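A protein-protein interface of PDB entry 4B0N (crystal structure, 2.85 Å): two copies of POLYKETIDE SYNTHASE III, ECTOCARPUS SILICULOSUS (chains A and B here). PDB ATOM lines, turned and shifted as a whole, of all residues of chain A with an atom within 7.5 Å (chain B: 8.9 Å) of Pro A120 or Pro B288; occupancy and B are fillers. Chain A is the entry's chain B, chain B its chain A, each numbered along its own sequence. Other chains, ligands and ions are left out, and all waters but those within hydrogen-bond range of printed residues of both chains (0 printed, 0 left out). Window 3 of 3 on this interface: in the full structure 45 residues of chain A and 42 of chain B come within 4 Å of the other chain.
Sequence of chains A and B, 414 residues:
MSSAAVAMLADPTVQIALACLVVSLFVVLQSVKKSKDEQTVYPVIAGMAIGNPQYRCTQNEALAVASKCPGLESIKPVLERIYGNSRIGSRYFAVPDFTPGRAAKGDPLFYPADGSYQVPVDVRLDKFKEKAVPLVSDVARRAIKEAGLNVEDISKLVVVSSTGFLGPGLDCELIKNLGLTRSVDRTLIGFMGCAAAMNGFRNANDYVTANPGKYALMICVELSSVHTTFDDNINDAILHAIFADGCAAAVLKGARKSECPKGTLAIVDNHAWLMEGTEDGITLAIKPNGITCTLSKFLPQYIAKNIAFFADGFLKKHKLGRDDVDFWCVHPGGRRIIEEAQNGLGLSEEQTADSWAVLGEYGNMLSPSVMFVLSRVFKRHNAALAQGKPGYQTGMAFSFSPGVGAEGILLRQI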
ATOM      1  N   PHE A 110     -20.637  15.767  26.755  1.00  0.00           N
ATOM      2  CA  PHE A 110     -21.146  14.703  25.896  1.00  0.00           C
ATOM      3  C   PHE A 110     -20.738  14.864  24.435  1.00  0.00           C
ATOM      4  O   PHE A 110     -20.494  13.872  23.747  1.00  0.00           O
ATOM      5  CB  PHE A 110     -22.668  14.601  26.025  1.00  0.00           C
ATOM      6  CG  PHE A 110     -23.283  13.510  25.195  1.00  0.00           C
ATOM      7  CD1 PHE A 110     -22.849  12.190  25.312  1.00  0.00           C
ATOM      8  CD2 PHE A 110     -24.308  13.799  24.298  1.00  0.00           C
ATOM      9  CE1 PHE A 110     -23.418  11.185  24.541  1.00  0.00           C
ATOM     10  CE2 PHE A 110     -24.884  12.797  23.530  1.00  0.00           C
ATOM     11  CZ  PHE A 110     -24.440  11.488  23.652  1.00  0.00           C
ATOM     12  N   TYR A 117     -20.193  17.979  16.747  1.00  0.00           N
ATOM     13  CA  TYR A 117     -21.476  17.465  17.245  1.00  0.00           C
ATOM     14  C   TYR A 117     -21.904  16.178  16.537  1.00  0.00           C
ATOM     15  O   TYR A 117     -23.076  15.985  16.204  1.00  0.00           O
ATOM     16  CB  TYR A 117     -22.567  18.543  17.179  1.00  0.00           C
ATOM     17  CG  TYR A 117     -22.337  19.694  18.138  1.00  0.00           C
ATOM     18  CD1 TYR A 117     -21.579  20.805  17.759  1.00  0.00           C
ATOM     19  CD2 TYR A 117     -22.873  19.671  19.428  1.00  0.00           C
ATOM     20  CE1 TYR A 117     -21.363  21.858  18.634  1.00  0.00           C
ATOM     21  CE2 TYR A 117     -22.662  20.721  20.309  1.00  0.00           C
ATOM     22  CZ  TYR A 117     -21.905  21.811  19.908  1.00  0.00           C
ATOM     23  OH  TYR A 117     -21.691  22.857  20.779  1.00  0.00           O
ATOM     24  N   GLN A 118     -20.924  15.305  16.315  1.00  0.00           N
ATOM     25  CA  GLN A 118     -21.137  14.029  15.650  1.00  0.00           C
ATOM     26  C   GLN A 118     -21.074  12.883  16.658  1.00  0.00           C
ATOM     27  O   GLN A 118     -19.991  12.450  17.070  1.00  0.00           O
ATOM     28  CB  GLN A 118     -20.109  13.828  14.530  1.00  0.00           C
ATOM     29  CG  GLN A 118     -20.345  14.693  13.298  1.00  0.00           C
ATOM     30  CD  GLN A 118     -21.351  14.089  12.331  1.00  0.00           C
ATOM     31  OE1 GLN A 118     -21.192  12.953  11.878  1.00  0.00           O
ATOM     32  NE2 GLN A 118     -22.387  14.855  12.000  1.00  0.00           N
ATOM     33  N   VAL A 119     -22.253  12.419  17.065  1.00  0.00           N
ATOM     34  CA  VAL A 119     -22.389  11.277  17.961  1.00  0.00           C
ATOM     35  C   VAL A 119     -23.399  10.315  17.331  1.00  0.00           C
ATOM     36  O   VAL A 119     -24.471  10.748  16.907  1.00  0.00           O
ATOM     37  CB  VAL A 119     -22.858  11.714  19.369  1.00  0.00           C
ATOM     38  CG1 VAL A 119     -23.008  10.517  20.296  1.00  0.00           C
ATOM     39  CG2 VAL A 119     -21.892  12.723  19.975  1.00  0.00           C
ATOM     40  N   PRO A 120     -23.050   9.013  17.238  1.00  0.00           N
ATOM     41  CA  PRO A 120     -23.986   8.024  16.684  1.00  0.00           C
ATOM     42  C   PRO A 120     -25.270   7.893  17.510  1.00  0.00           C
ATOM     43  O   PRO A 120     -25.237   8.031  18.738  1.00  0.00           O
ATOM     44  CB  PRO A 120     -23.181   6.714  16.703  1.00  0.00           C
ATOM     45  CG  PRO A 120     -22.021   6.959  17.605  1.00  0.00           C
ATOM     46  CD  PRO A 120     -21.729   8.422  17.520  1.00  0.00           C
ATOM     47  N   VAL A 121     -26.384   7.627  16.830  1.00  0.00           N
ATOM     48  CA  VAL A 121     -27.718   7.669  17.441  1.00  0.00           C
ATOM     49  C   VAL A 121     -27.902   6.709  18.628  1.00  0.00           C
ATOM     50  O   VAL A 121     -28.576   7.047  19.602  1.00  0.00           O
ATOM     51  CB  VAL A 121     -28.843   7.512  16.378  1.00  0.00           C
ATOM     52  CG1 VAL A 121     -28.878   6.106  15.796  1.00  0.00           C
ATOM     53  CG2 VAL A 121     -30.199   7.908  16.947  1.00  0.00           C
ATOM     54  N   ASP A 122     -27.284   5.531  18.551  1.00  0.00           N
ATOM     55  CA  ASP A 122     -27.344   4.542  19.636  1.00  0.00           C
ATOM     56  C   ASP A 122     -26.626   5.017  20.902  1.00  0.00           C
ATOM     57  O   ASP A 122     -27.070   4.732  22.016  1.00  0.00           O
ATOM     58  CB  ASP A 122     -26.784   3.189  19.175  1.00  0.00           C
ATOM     59  CG  ASP A 122     -25.339   3.276  18.707  1.00  0.00           C
ATOM     60  OD1 ASP A 122     -24.989   4.249  18.002  1.00  0.00           O
ATOM     61  OD2 ASP A 122     -24.551   2.364  19.044  1.00  0.00           O
ATOM     62  N   VAL A 123     -25.524   5.744  20.720  1.00  0.00           N
ATOM     63  CA  VAL A 123     -24.769   6.323  21.833  1.00  0.00           C
ATOM     64  C   VAL A 123     -25.586   7.443  22.478  1.00  0.00           C
ATOM     65  O   VAL A 123     -25.530   7.646  23.695  1.00  0.00           O
ATOM     66  CB  VAL A 123     -23.382   6.837  21.374  1.00  0.00           C
ATOM     67  CG1 VAL A 123     -22.639   7.525  22.513  1.00  0.00           C
ATOM     68  CG2 VAL A 123     -22.544   5.691  20.824  1.00  0.00           C
ATOM     69  N   ARG A 124     -26.353   8.152  21.651  1.00  0.00           N
ATOM     70  CA  ARG A 124     -27.243   9.212  22.116  1.00  0.00           C
ATOM     71  C   ARG A 124     -28.363   8.633  22.969  1.00  0.00           C
ATOM     72  O   ARG A 124     -28.724   9.205  23.998  1.00  0.00           O
ATOM     73  CB  ARG A 124     -27.823   9.992  20.933  1.00  0.00           C
ATOM     74  CG  ARG A 124     -26.808  10.853  20.194  1.00  0.00           C
ATOM     75  CD  ARG A 124     -27.409  11.469  18.943  1.00  0.00           C
ATOM     76  NE  ARG A 124     -26.427  12.235  18.177  1.00  0.00           N
ATOM     77  CZ  ARG A 124     -26.236  13.546  18.292  1.00  0.00           C
ATOM     78  NH1 ARG A 124     -26.963  14.259  19.142  1.00  0.00           N
ATOM     79  NH2 ARG A 124     -25.320  14.150  17.547  1.00  0.00           N
ATOM     80  N   LEU A 125     -28.898   7.491  22.545  1.00  0.00           N
ATOM     81  CA  LEU A 125     -29.958   6.821  23.292  1.00  0.00           C
ATOM     82  C   LEU A 125     -29.428   6.235  24.596  1.00  0.00           C
ATOM     83  O   LEU A 125     -30.155   6.181  25.586  1.00  0.00           O
ATOM     84  CB  LEU A 125     -30.649   5.749  22.443  1.00  0.00           C
ATOM     85  CG  LEU A 125     -31.418   6.236  21.207  1.00  0.00           C
ATOM     86  CD1 LEU A 125     -31.941   5.058  20.399  1.00  0.00           C
ATOM     87  CD2 LEU A 125     -32.556   7.183  21.567  1.00  0.00           C
ATOM     88  N   ASP A 126     -28.162   5.815  24.593  1.00  0.00           N
ATOM     89  CA  ASP A 126     -27.481   5.375  25.811  1.00  0.00           C
ATOM     90  C   ASP A 126     -27.404   6.487  26.851  1.00  0.00           C
ATOM     91  O   ASP A 126     -27.607   6.238  28.038  1.00  0.00           O
ATOM     92  CB  ASP A 126     -26.073   4.856  25.498  1.00  0.00           C
ATOM     93  CG  ASP A 126     -26.051   3.373  25.157  1.00  0.00           C
ATOM     94  OD1 ASP A 126     -26.874   2.605  25.706  1.00  0.00           O
ATOM     95  OD2 ASP A 126     -25.190   2.975  24.343  1.00  0.00           O
ATOM     96  N   VAL A 226     -29.949  15.584  24.039  1.00  0.00           N
ATOM     97  CA  VAL A 226     -29.192  14.428  23.573  1.00  0.00           C
ATOM     98  C   VAL A 226     -29.132  14.368  22.035  1.00  0.00           C
ATOM     99  O   VAL A 226     -28.226  13.756  21.463  1.00  0.00           O
ATOM    100  CB  VAL A 226     -29.759  13.131  24.210  1.00  0.00           C
ATOM    101  CG1 VAL A 226     -30.029  12.041  23.184  1.00  0.00           C
ATOM    102  CG2 VAL A 226     -28.841  12.636  25.320  1.00  0.00           C
ATOM    103  N   ILE A 286     -35.895   9.419  12.541  1.00  0.00           N
ATOM    104  CA  ILE A 286     -34.722   8.960  13.268  1.00  0.00           C
ATOM    105  C   ILE A 286     -33.577   8.838  12.274  1.00  0.00           C
ATOM    106  O   ILE A 286     -33.667   8.095  11.297  1.00  0.00           O
ATOM    107  CB  ILE A 286     -34.948   7.611  13.975  1.00  0.00           C
ATOM    108  CG1 ILE A 286     -36.284   7.613  14.725  1.00  0.00           C
ATOM    109  CG2 ILE A 286     -33.788   7.322  14.920  1.00  0.00           C
ATOM    110  CD1 ILE A 286     -36.641   6.289  15.371  1.00  0.00           C
ATOM    111  N   LYS A 287     -32.513   9.589  12.524  1.00  0.00           N
ATOM    112  CA  LYS A 287     -31.352   9.618  11.643  1.00  0.00           C
ATOM    113  C   LYS A 287     -30.097   9.192  12.413  1.00  0.00           C
ATOM    114  O   LYS A 287     -30.093   9.223  13.647  1.00  0.00           O
ATOM    115  CB  LYS A 287     -31.190  11.018  11.037  1.00  0.00           C
ATOM    116  CG  LYS A 287     -32.399  11.495  10.246  1.00  0.00           C
ATOM    117  CD  LYS A 287     -32.080  12.703   9.384  1.00  0.00           C
ATOM    118  CE  LYS A 287     -33.292  13.109   8.564  1.00  0.00           C
ATOM    119  NZ  LYS A 287     -33.055  14.369   7.810  1.00  0.00           N
ATOM    120  N   PRO A 288     -29.030   8.784  11.694  1.00  0.00           N
ATOM    121  CA  PRO A 288     -27.791   8.347  12.353  1.00  0.00           C
ATOM    122  C   PRO A 288     -27.227   9.325  13.395  1.00  0.00           C
ATOM    123  O   PRO A 288     -26.624   8.890  14.377  1.00  0.00           O
ATOM    124  CB  PRO A 288     -26.816   8.192  11.182  1.00  0.00           C
ATOM    125  CG  PRO A 288     -27.687   7.829  10.033  1.00  0.00           C
ATOM    126  CD  PRO A 288     -28.952   8.617  10.229  1.00  0.00           C
ATOM    127  N   ASN A 289     -27.425  10.624  13.180  1.00  0.00           N
ATOM    128  CA  ASN A 289     -26.898  11.641  14.087  1.00  0.00           C
ATOM    129  C   ASN A 289     -27.925  12.150  15.105  1.00  0.00           C
ATOM    130  O   ASN A 289     -27.715  13.181  15.745  1.00  0.00           O
ATOM    131  CB  ASN A 289     -26.285  12.802  13.294  1.00  0.00           C
ATOM    132  CG  ASN A 289     -25.275  13.599  14.104  1.00  0.00           C
ATOM    133  OD1 ASN A 289     -24.699  13.101  15.075  1.00  0.00           O
ATOM    134  ND2 ASN A 289     -25.052  14.847  13.703  1.00  0.00           N
ATOM    135  N   GLY A 290     -29.029  11.421  15.255  1.00  0.00           N
ATOM    136  CA  GLY A 290     -30.021  11.729  16.282  1.00  0.00           C
ATOM    137  C   GLY A 290     -31.454  11.771  15.795  1.00  0.00           C
ATOM    138  O   GLY A 290     -31.716  11.834  14.590  1.00  0.00           O
ATOM    139  N   TYR B 117     -24.705  -4.105   2.793  1.00  0.00           N
ATOM    140  CA  TYR B 117     -25.891  -3.846   3.620  1.00  0.00           C
ATOM    141  C   TYR B 117     -25.711  -2.621   4.531  1.00  0.00           C
ATOM    142  O   TYR B 117     -25.912  -2.686   5.747  1.00  0.00           O
ATOM    143  CB  TYR B 117     -26.306  -5.113   4.393  1.00  0.00           C
ATOM    144  CG  TYR B 117     -26.700  -6.255   3.480  1.00  0.00           C
ATOM    145  CD1 TYR B 117     -25.741  -7.136   2.971  1.00  0.00           C
ATOM    146  CD2 TYR B 117     -28.031  -6.444   3.103  1.00  0.00           C
ATOM    147  CE1 TYR B 117     -26.098  -8.175   2.122  1.00  0.00           C
ATOM    148  CE2 TYR B 117     -28.397  -7.480   2.254  1.00  0.00           C
ATOM    149  CZ  TYR B 117     -27.430  -8.342   1.768  1.00  0.00           C
ATOM    150  OH  TYR B 117     -27.796  -9.369   0.927  1.00  0.00           O
ATOM    151  N   GLN B 118     -25.322  -1.509   3.910  1.00  0.00           N
ATOM    152  CA  GLN B 118     -25.121  -0.238   4.599  1.00  0.00           C
ATOM    153  C   GLN B 118     -26.211   0.732   4.165  1.00  0.00           C
ATOM    154  O   GLN B 118     -26.127   1.339   3.092  1.00  0.00           O
ATOM    155  CB  GLN B 118     -23.741   0.351   4.276  1.00  0.00           C
ATOM    156  CG  GLN B 118     -22.560  -0.568   4.557  1.00  0.00           C
ATOM    157  CD  GLN B 118     -22.106  -0.529   6.001  1.00  0.00           C
ATOM    158  OE1 GLN B 118     -21.639   0.501   6.492  1.00  0.00           O
ATOM    159  NE2 GLN B 118     -22.226  -1.661   6.688  1.00  0.00           N
ATOM    160  N   VAL B 119     -27.248   0.850   4.990  1.00  0.00           N
ATOM    161  CA  VAL B 119     -28.343   1.785   4.746  1.00  0.00           C
ATOM    162  C   VAL B 119     -28.629   2.576   6.025  1.00  0.00           C
ATOM    163  O   VAL B 119     -28.790   1.984   7.096  1.00  0.00           O
ATOM    164  CB  VAL B 119     -29.630   1.073   4.274  1.00  0.00           C
ATOM    165  CG1 VAL B 119     -30.697   2.090   3.906  1.00  0.00           C
ATOM    166  CG2 VAL B 119     -29.350   0.165   3.085  1.00  0.00           C
ATOM    167  N   PRO B 120     -28.675   3.918   5.923  1.00  0.00           N
ATOM    168  CA  PRO B 120     -28.994   4.766   7.072  1.00  0.00           C
ATOM    169  C   PRO B 120     -30.395   4.487   7.620  1.00  0.00           C
ATOM    170  O   PRO B 120     -31.296   4.146   6.843  1.00  0.00           O
ATOM    171  CB  PRO B 120     -28.920   6.179   6.487  1.00  0.00           C
ATOM    172  CG  PRO B 120     -27.987   6.056   5.335  1.00  0.00           C
ATOM    173  CD  PRO B 120     -28.297   4.719   4.744  1.00  0.00           C
ATOM    174  N   VAL B 121     -30.565   4.632   8.940  1.00  0.00           N
ATOM    175  CA  VAL B 121     -31.846   4.359   9.612  1.00  0.00           C
ATOM    176  C   VAL B 121     -33.034   5.079   8.997  1.00  0.00           C
ATOM    177  O   VAL B 121     -34.103   4.488   8.854  1.00  0.00           O
ATOM    178  CB  VAL B 121     -31.843   4.682  11.128  1.00  0.00           C
ATOM    179  CG1 VAL B 121     -31.933   3.410  11.956  1.00  0.00           C
ATOM    180  CG2 VAL B 121     -30.658   5.550  11.527  1.00  0.00           C
ATOM    181  N   ASP B 122     -32.852   6.349   8.650  1.00  0.00           N
ATOM    182  CA  ASP B 122     -33.949   7.140   8.096  1.00  0.00           C
ATOM    183  C   ASP B 122     -34.450   6.579   6.766  1.00  0.00           C
ATOM    184  O   ASP B 122     -35.659   6.527   6.537  1.00  0.00           O
ATOM    185  CB  ASP B 122     -33.589   8.630   7.989  1.00  0.00           C
ATOM    186  CG  ASP B 122     -32.278   8.877   7.271  1.00  0.00           C
ATOM    187  OD1 ASP B 122     -31.252   8.266   7.647  1.00  0.00           O
ATOM    188  OD2 ASP B 122     -32.276   9.705   6.337  1.00  0.00           O
ATOM    189  N   VAL B 123     -33.523   6.138   5.913  1.00  0.00           N
ATOM    190  CA  VAL B 123     -33.870   5.504   4.634  1.00  0.00           C
ATOM    191  C   VAL B 123     -34.552   4.150   4.868  1.00  0.00           C
ATOM    192  O   VAL B 123     -35.512   3.802   4.173  1.00  0.00           O
ATOM    193  CB  VAL B 123     -32.635   5.337   3.717  1.00  0.00           C
ATOM    194  CG1 VAL B 123     -33.040   4.845   2.332  1.00  0.00           C
ATOM    195  CG2 VAL B 123     -31.868   6.647   3.602  1.00  0.00           C
ATOM    196  N   ARG B 124     -34.057   3.403   5.856  1.00  0.00           N
ATOM    197  CA  ARG B 124     -34.668   2.135   6.268  1.00  0.00           C
ATOM    198  C   ARG B 124     -36.099   2.328   6.777  1.00  0.00           C
ATOM    199  O   ARG B 124     -36.989   1.536   6.460  1.00  0.00           O
ATOM    200  CB  ARG B 124     -33.814   1.430   7.330  1.00  0.00           C
ATOM    201  CG  ARG B 124     -32.534   0.816   6.786  1.00  0.00           C
ATOM    202  CD  ARG B 124     -31.737   0.098   7.865  1.00  0.00           C
ATOM    203  NE  ARG B 124     -30.396  -0.256   7.399  1.00  0.00           N
ATOM    204  CZ  ARG B 124     -30.033  -1.452   6.937  1.00  0.00           C
ATOM    205  NH1 ARG B 124     -30.899  -2.456   6.876  1.00  0.00           N
ATOM    206  NH2 ARG B 124     -28.785  -1.649   6.539  1.00  0.00           N
ATOM    207  N   LEU B 125     -36.314   3.387   7.556  1.00  0.00           N
ATOM    208  CA  LEU B 125     -37.644   3.695   8.088  1.00  0.00           C
ATOM    209  C   LEU B 125     -38.579   4.271   7.020  1.00  0.00           C
ATOM    210  O   LEU B 125     -39.789   4.052   7.071  1.00  0.00           O
ATOM    211  CB  LEU B 125     -37.551   4.619   9.312  1.00  0.00           C
ATOM    212  CG  LEU B 125     -36.968   3.994  10.586  1.00  0.00           C
ATOM    213  CD1 LEU B 125     -36.503   5.067  11.555  1.00  0.00           C
ATOM    214  CD2 LEU B 125     -37.957   3.047  11.254  1.00  0.00           C
ATOM    215  N   HIS B 227     -34.243  -4.020   8.126  1.00  0.00           N
ATOM    216  CA  HIS B 227     -33.172  -3.786   9.098  1.00  0.00           C
ATOM    217  C   HIS B 227     -32.019  -4.750   8.988  1.00  0.00           C
ATOM    218  O   HIS B 227     -31.204  -4.856   9.909  1.00  0.00           O
ATOM    219  CB  HIS B 227     -33.735  -3.805  10.516  1.00  0.00           C
ATOM    220  CG  HIS B 227     -34.764  -2.735  10.774  1.00  0.00           C
ATOM    221  ND1 HIS B 227     -34.436  -1.438  10.914  1.00  0.00           N
ATOM    222  CD2 HIS B 227     -36.148  -2.810  10.912  1.00  0.00           C
ATOM    223  CE1 HIS B 227     -35.551  -0.716  11.127  1.00  0.00           C
ATOM    224  NE2 HIS B 227     -36.598  -1.558  11.128  1.00  0.00           N
ATOM    225  N   THR B 229     -28.498  -6.362   8.113  1.00  0.00           N
ATOM    226  CA  THR B 229     -27.145  -5.800   8.094  1.00  0.00           C
ATOM    227  C   THR B 229     -26.087  -6.829   7.706  1.00  0.00           C
ATOM    228  O   THR B 229     -25.007  -6.467   7.225  1.00  0.00           O
ATOM    229  CB  THR B 229     -26.753  -5.214   9.465  1.00  0.00           C
ATOM    230  OG1 THR B 229     -26.824  -6.239  10.459  1.00  0.00           O
ATOM    231  CG2 THR B 229     -27.671  -4.068   9.857  1.00  0.00           C
ATOM    232  N   ALA B 285     -31.780  -2.096  20.275  1.00  0.00           N
ATOM    233  CA  ALA B 285     -31.103  -0.829  20.023  1.00  0.00           C
ATOM    234  C   ALA B 285     -31.496  -0.238  18.679  1.00  0.00           C
ATOM    235  O   ALA B 285     -31.920  -0.957  17.772  1.00  0.00           O
ATOM    236  CB  ALA B 285     -29.592  -1.008  20.106  1.00  0.00           C
ATOM    237  N   ILE B 286     -31.368   1.080  18.568  1.00  0.00           N
ATOM    238  CA  ILE B 286     -31.446   1.747  17.279  1.00  0.00           C
ATOM    239  C   ILE B 286     -30.063   2.288  16.939  1.00  0.00           C
ATOM    240  O   ILE B 286     -29.638   3.312  17.474  1.00  0.00           O
ATOM    241  CB  ILE B 286     -32.477   2.894  17.258  1.00  0.00           C
ATOM    242  CG1 ILE B 286     -33.817   2.436  17.845  1.00  0.00           C
ATOM    243  CG2 ILE B 286     -32.648   3.414  15.835  1.00  0.00           C
ATOM    244  CD1 ILE B 286     -34.795   3.566  18.086  1.00  0.00           C
ATOM    245  N   LYS B 287     -29.362   1.576  16.063  1.00  0.00           N
ATOM    246  CA  LYS B 287     -28.042   1.981  15.592  1.00  0.00           C
ATOM    247  C   LYS B 287     -28.169   2.743  14.266  1.00  0.00           C
ATOM    248  O   LYS B 287     -29.223   2.692  13.631  1.00  0.00           O
ATOM    249  CB  LYS B 287     -27.141   0.751  15.435  1.00  0.00           C
ATOM    250  CG  LYS B 287     -26.683   0.146  16.752  1.00  0.00           C
ATOM    251  CD  LYS B 287     -25.991  -1.192  16.550  1.00  0.00           C
ATOM    252  CE  LYS B 287     -25.528  -1.772  17.881  1.00  0.00           C
ATOM    253  NZ  LYS B 287     -24.998  -3.157  17.744  1.00  0.00           N
ATOM    254  N   PRO B 288     -27.106   3.466  13.849  1.00  0.00           N
ATOM    255  CA  PRO B 288     -27.126   4.182  12.566  1.00  0.00           C
ATOM    256  C   PRO B 288     -27.438   3.308  11.342  1.00  0.00           C
ATOM    257  O   PRO B 288     -28.025   3.801  10.375  1.00  0.00           O
ATOM    258  CB  PRO B 288     -25.708   4.745  12.465  1.00  0.00           C
ATOM    259  CG  PRO B 288     -25.293   4.944  13.880  1.00  0.00           C
ATOM    260  CD  PRO B 288     -25.894   3.789  14.629  1.00  0.00           C
ATOM    261  N   ASN B 289     -27.054   2.033  11.381  1.00  0.00           N
ATOM    262  CA  ASN B 289     -27.307   1.126  10.259  1.00  0.00           C
ATOM    263  C   ASN B 289     -28.596   0.306  10.405  1.00  0.00           C
ATOM    264  O   ASN B 289     -28.768  -0.733   9.757  1.00  0.00           O
ATOM    265  CB  ASN B 289     -26.099   0.214  10.015  1.00  0.00           C
ATOM    266  CG  ASN B 289     -26.087  -0.380   8.618  1.00  0.00           C
ATOM    267  OD1 ASN B 289     -26.543   0.240   7.656  1.00  0.00           O
ATOM    268  ND2 ASN B 289     -25.555  -1.591   8.500  1.00  0.00           N
ATOM    269  N   GLY B 290     -29.504   0.783  11.250  1.00  0.00           N
ATOM    270  CA  GLY B 290     -30.794   0.132  11.439  1.00  0.00           C
ATOM    271  C   GLY B 290     -31.079  -0.260  12.873  1.00  0.00           C
ATOM    272  O   GLY B 290     -30.190  -0.219  13.729  1.00  0.00           O
ATOM    273  N   ILE B 291     -32.333  -0.631  13.131  1.00  0.00           N
ATOM    274  CA  ILE B 291     -32.746  -1.165  14.425  1.00  0.00           C
ATOM    275  C   ILE B 291     -32.242  -2.600  14.534  1.00  0.00           C
ATOM    276  O   ILE B 291     -32.463  -3.413  13.631  1.00  0.00           O
ATOM    277  CB  ILE B 291     -34.281  -1.136  14.588  1.00  0.00           C
ATOM    278  CG1 ILE B 291     -34.794   0.309  14.539  1.00  0.00           C
ATOM    279  CG2 ILE B 291     -34.694  -1.822  15.884  1.00  0.00           C
ATOM    280  CD1 ILE B 291     -36.287   0.442  14.331  1.00  0.00           C
ATOM    281  N   THR B 292     -31.549  -2.904  15.626  1.00  0.00           N
ATOM    282  CA  THR B 292     -31.043  -4.256  15.844  1.00  0.00           C
ATOM    283  C   THR B 292     -31.610  -4.922  17.083  1.00  0.00           C
ATOM    284  O   THR B 292     -32.072  -4.270  18.026  1.00  0.00           O
ATOM    285  CB  THR B 292     -29.505  -4.316  15.919  1.00  0.00           C
ATOM    286  OG1 THR B 292     -29.014  -3.222  16.705  1.00  0.00           O
ATOM    287  CG2 THR B 292     -28.897  -4.270  14.522  1.00  0.00           C
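N of Asp A122 lies close to O of Ile B286 (3.4 Å). The backbone carbonyl oxygen (O) of Ile A286 lies within hydrogen-bond range of the backbone NH (N) of Asp B122, 3.3 Å away.
O of Pro A288 sits at hydrogen-bond distance from N of Val A121 (2.8 Å). O of Pro B288 lies within hydrogen-bond range of N of Val B121, at 3.0 Å.
Among the printed residues, pairs that only touch across the chains: Val A121 with Ile B286 (3.3 Å), Pro A288 with Asp B122 (3.5 Å), Asp A122 with Pro B288 (3.5 Å), Pro A288 with Val B121 (3.6 Å), Val A121 with Pro B288 (3.7 Å), Val A121 with Lys B287 (3.8 Å), Lys A287 with Val B121 (3.8 Å), Asp A122 with Lys B287 (3.8 Å), Lys A287 with Asp B122 (3.8 Å), Ile A286 with Leu B125 (3.8 Å), Pro A288 with Pro B288 (3.8 Å), Ile A286 with Val B121 (3.8 Å), Leu A125 with Ile B286 (3.9 Å) and Pro A120 with Pro B288 (3.9 Å).
Pro A120 touches one residue of chain B. Of chain A, only Pro A120 (3.9 Å), Val A121 (3.7 Å), Asp A122 (3.5 Å) and Pro A288 (3.8 Å) come within 4 Å of Pro B288. No residue of chain B comes within 4 Å of Val A119. Printed residues of chain A within 4 Å of Leu B125: Ile A286 (3.8 Å). Of the printed residues of chain B, Pro A288 touches Val B121 (3.6 Å), Asp B122 (3.5 Å) and Pro B288 (3.8 Å). The nearest residue of chain B that does not touch Pro A120 is Ile B286 (6.3 Å).
Of the 19 printed residues of chain B, 6 touch a printed residue of chain A. Printed residues of chain B that touch a printed residue of chain A: Val B121, Asp B122, Leu B125, Ile B286, Lys B287 and Pro B288.
Pro A120 touches Pro B288, but with the chains exchanged Pro A288 does not touch Pro B120 (4.1 Å). Val A121 touches Ile B286, and with the chains exchanged Ile A286 touches Val B121. Leu A125 touches Ile B286, and with the chains exchanged Ile A286 touches Leu B125. Pro A288 touches its own counterpart, Pro B288. 14 positions are printed for both chains. Of the 16 pairs that touch across the chains among the printed residues, 15 have their exchanged pair printed and touching as well.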
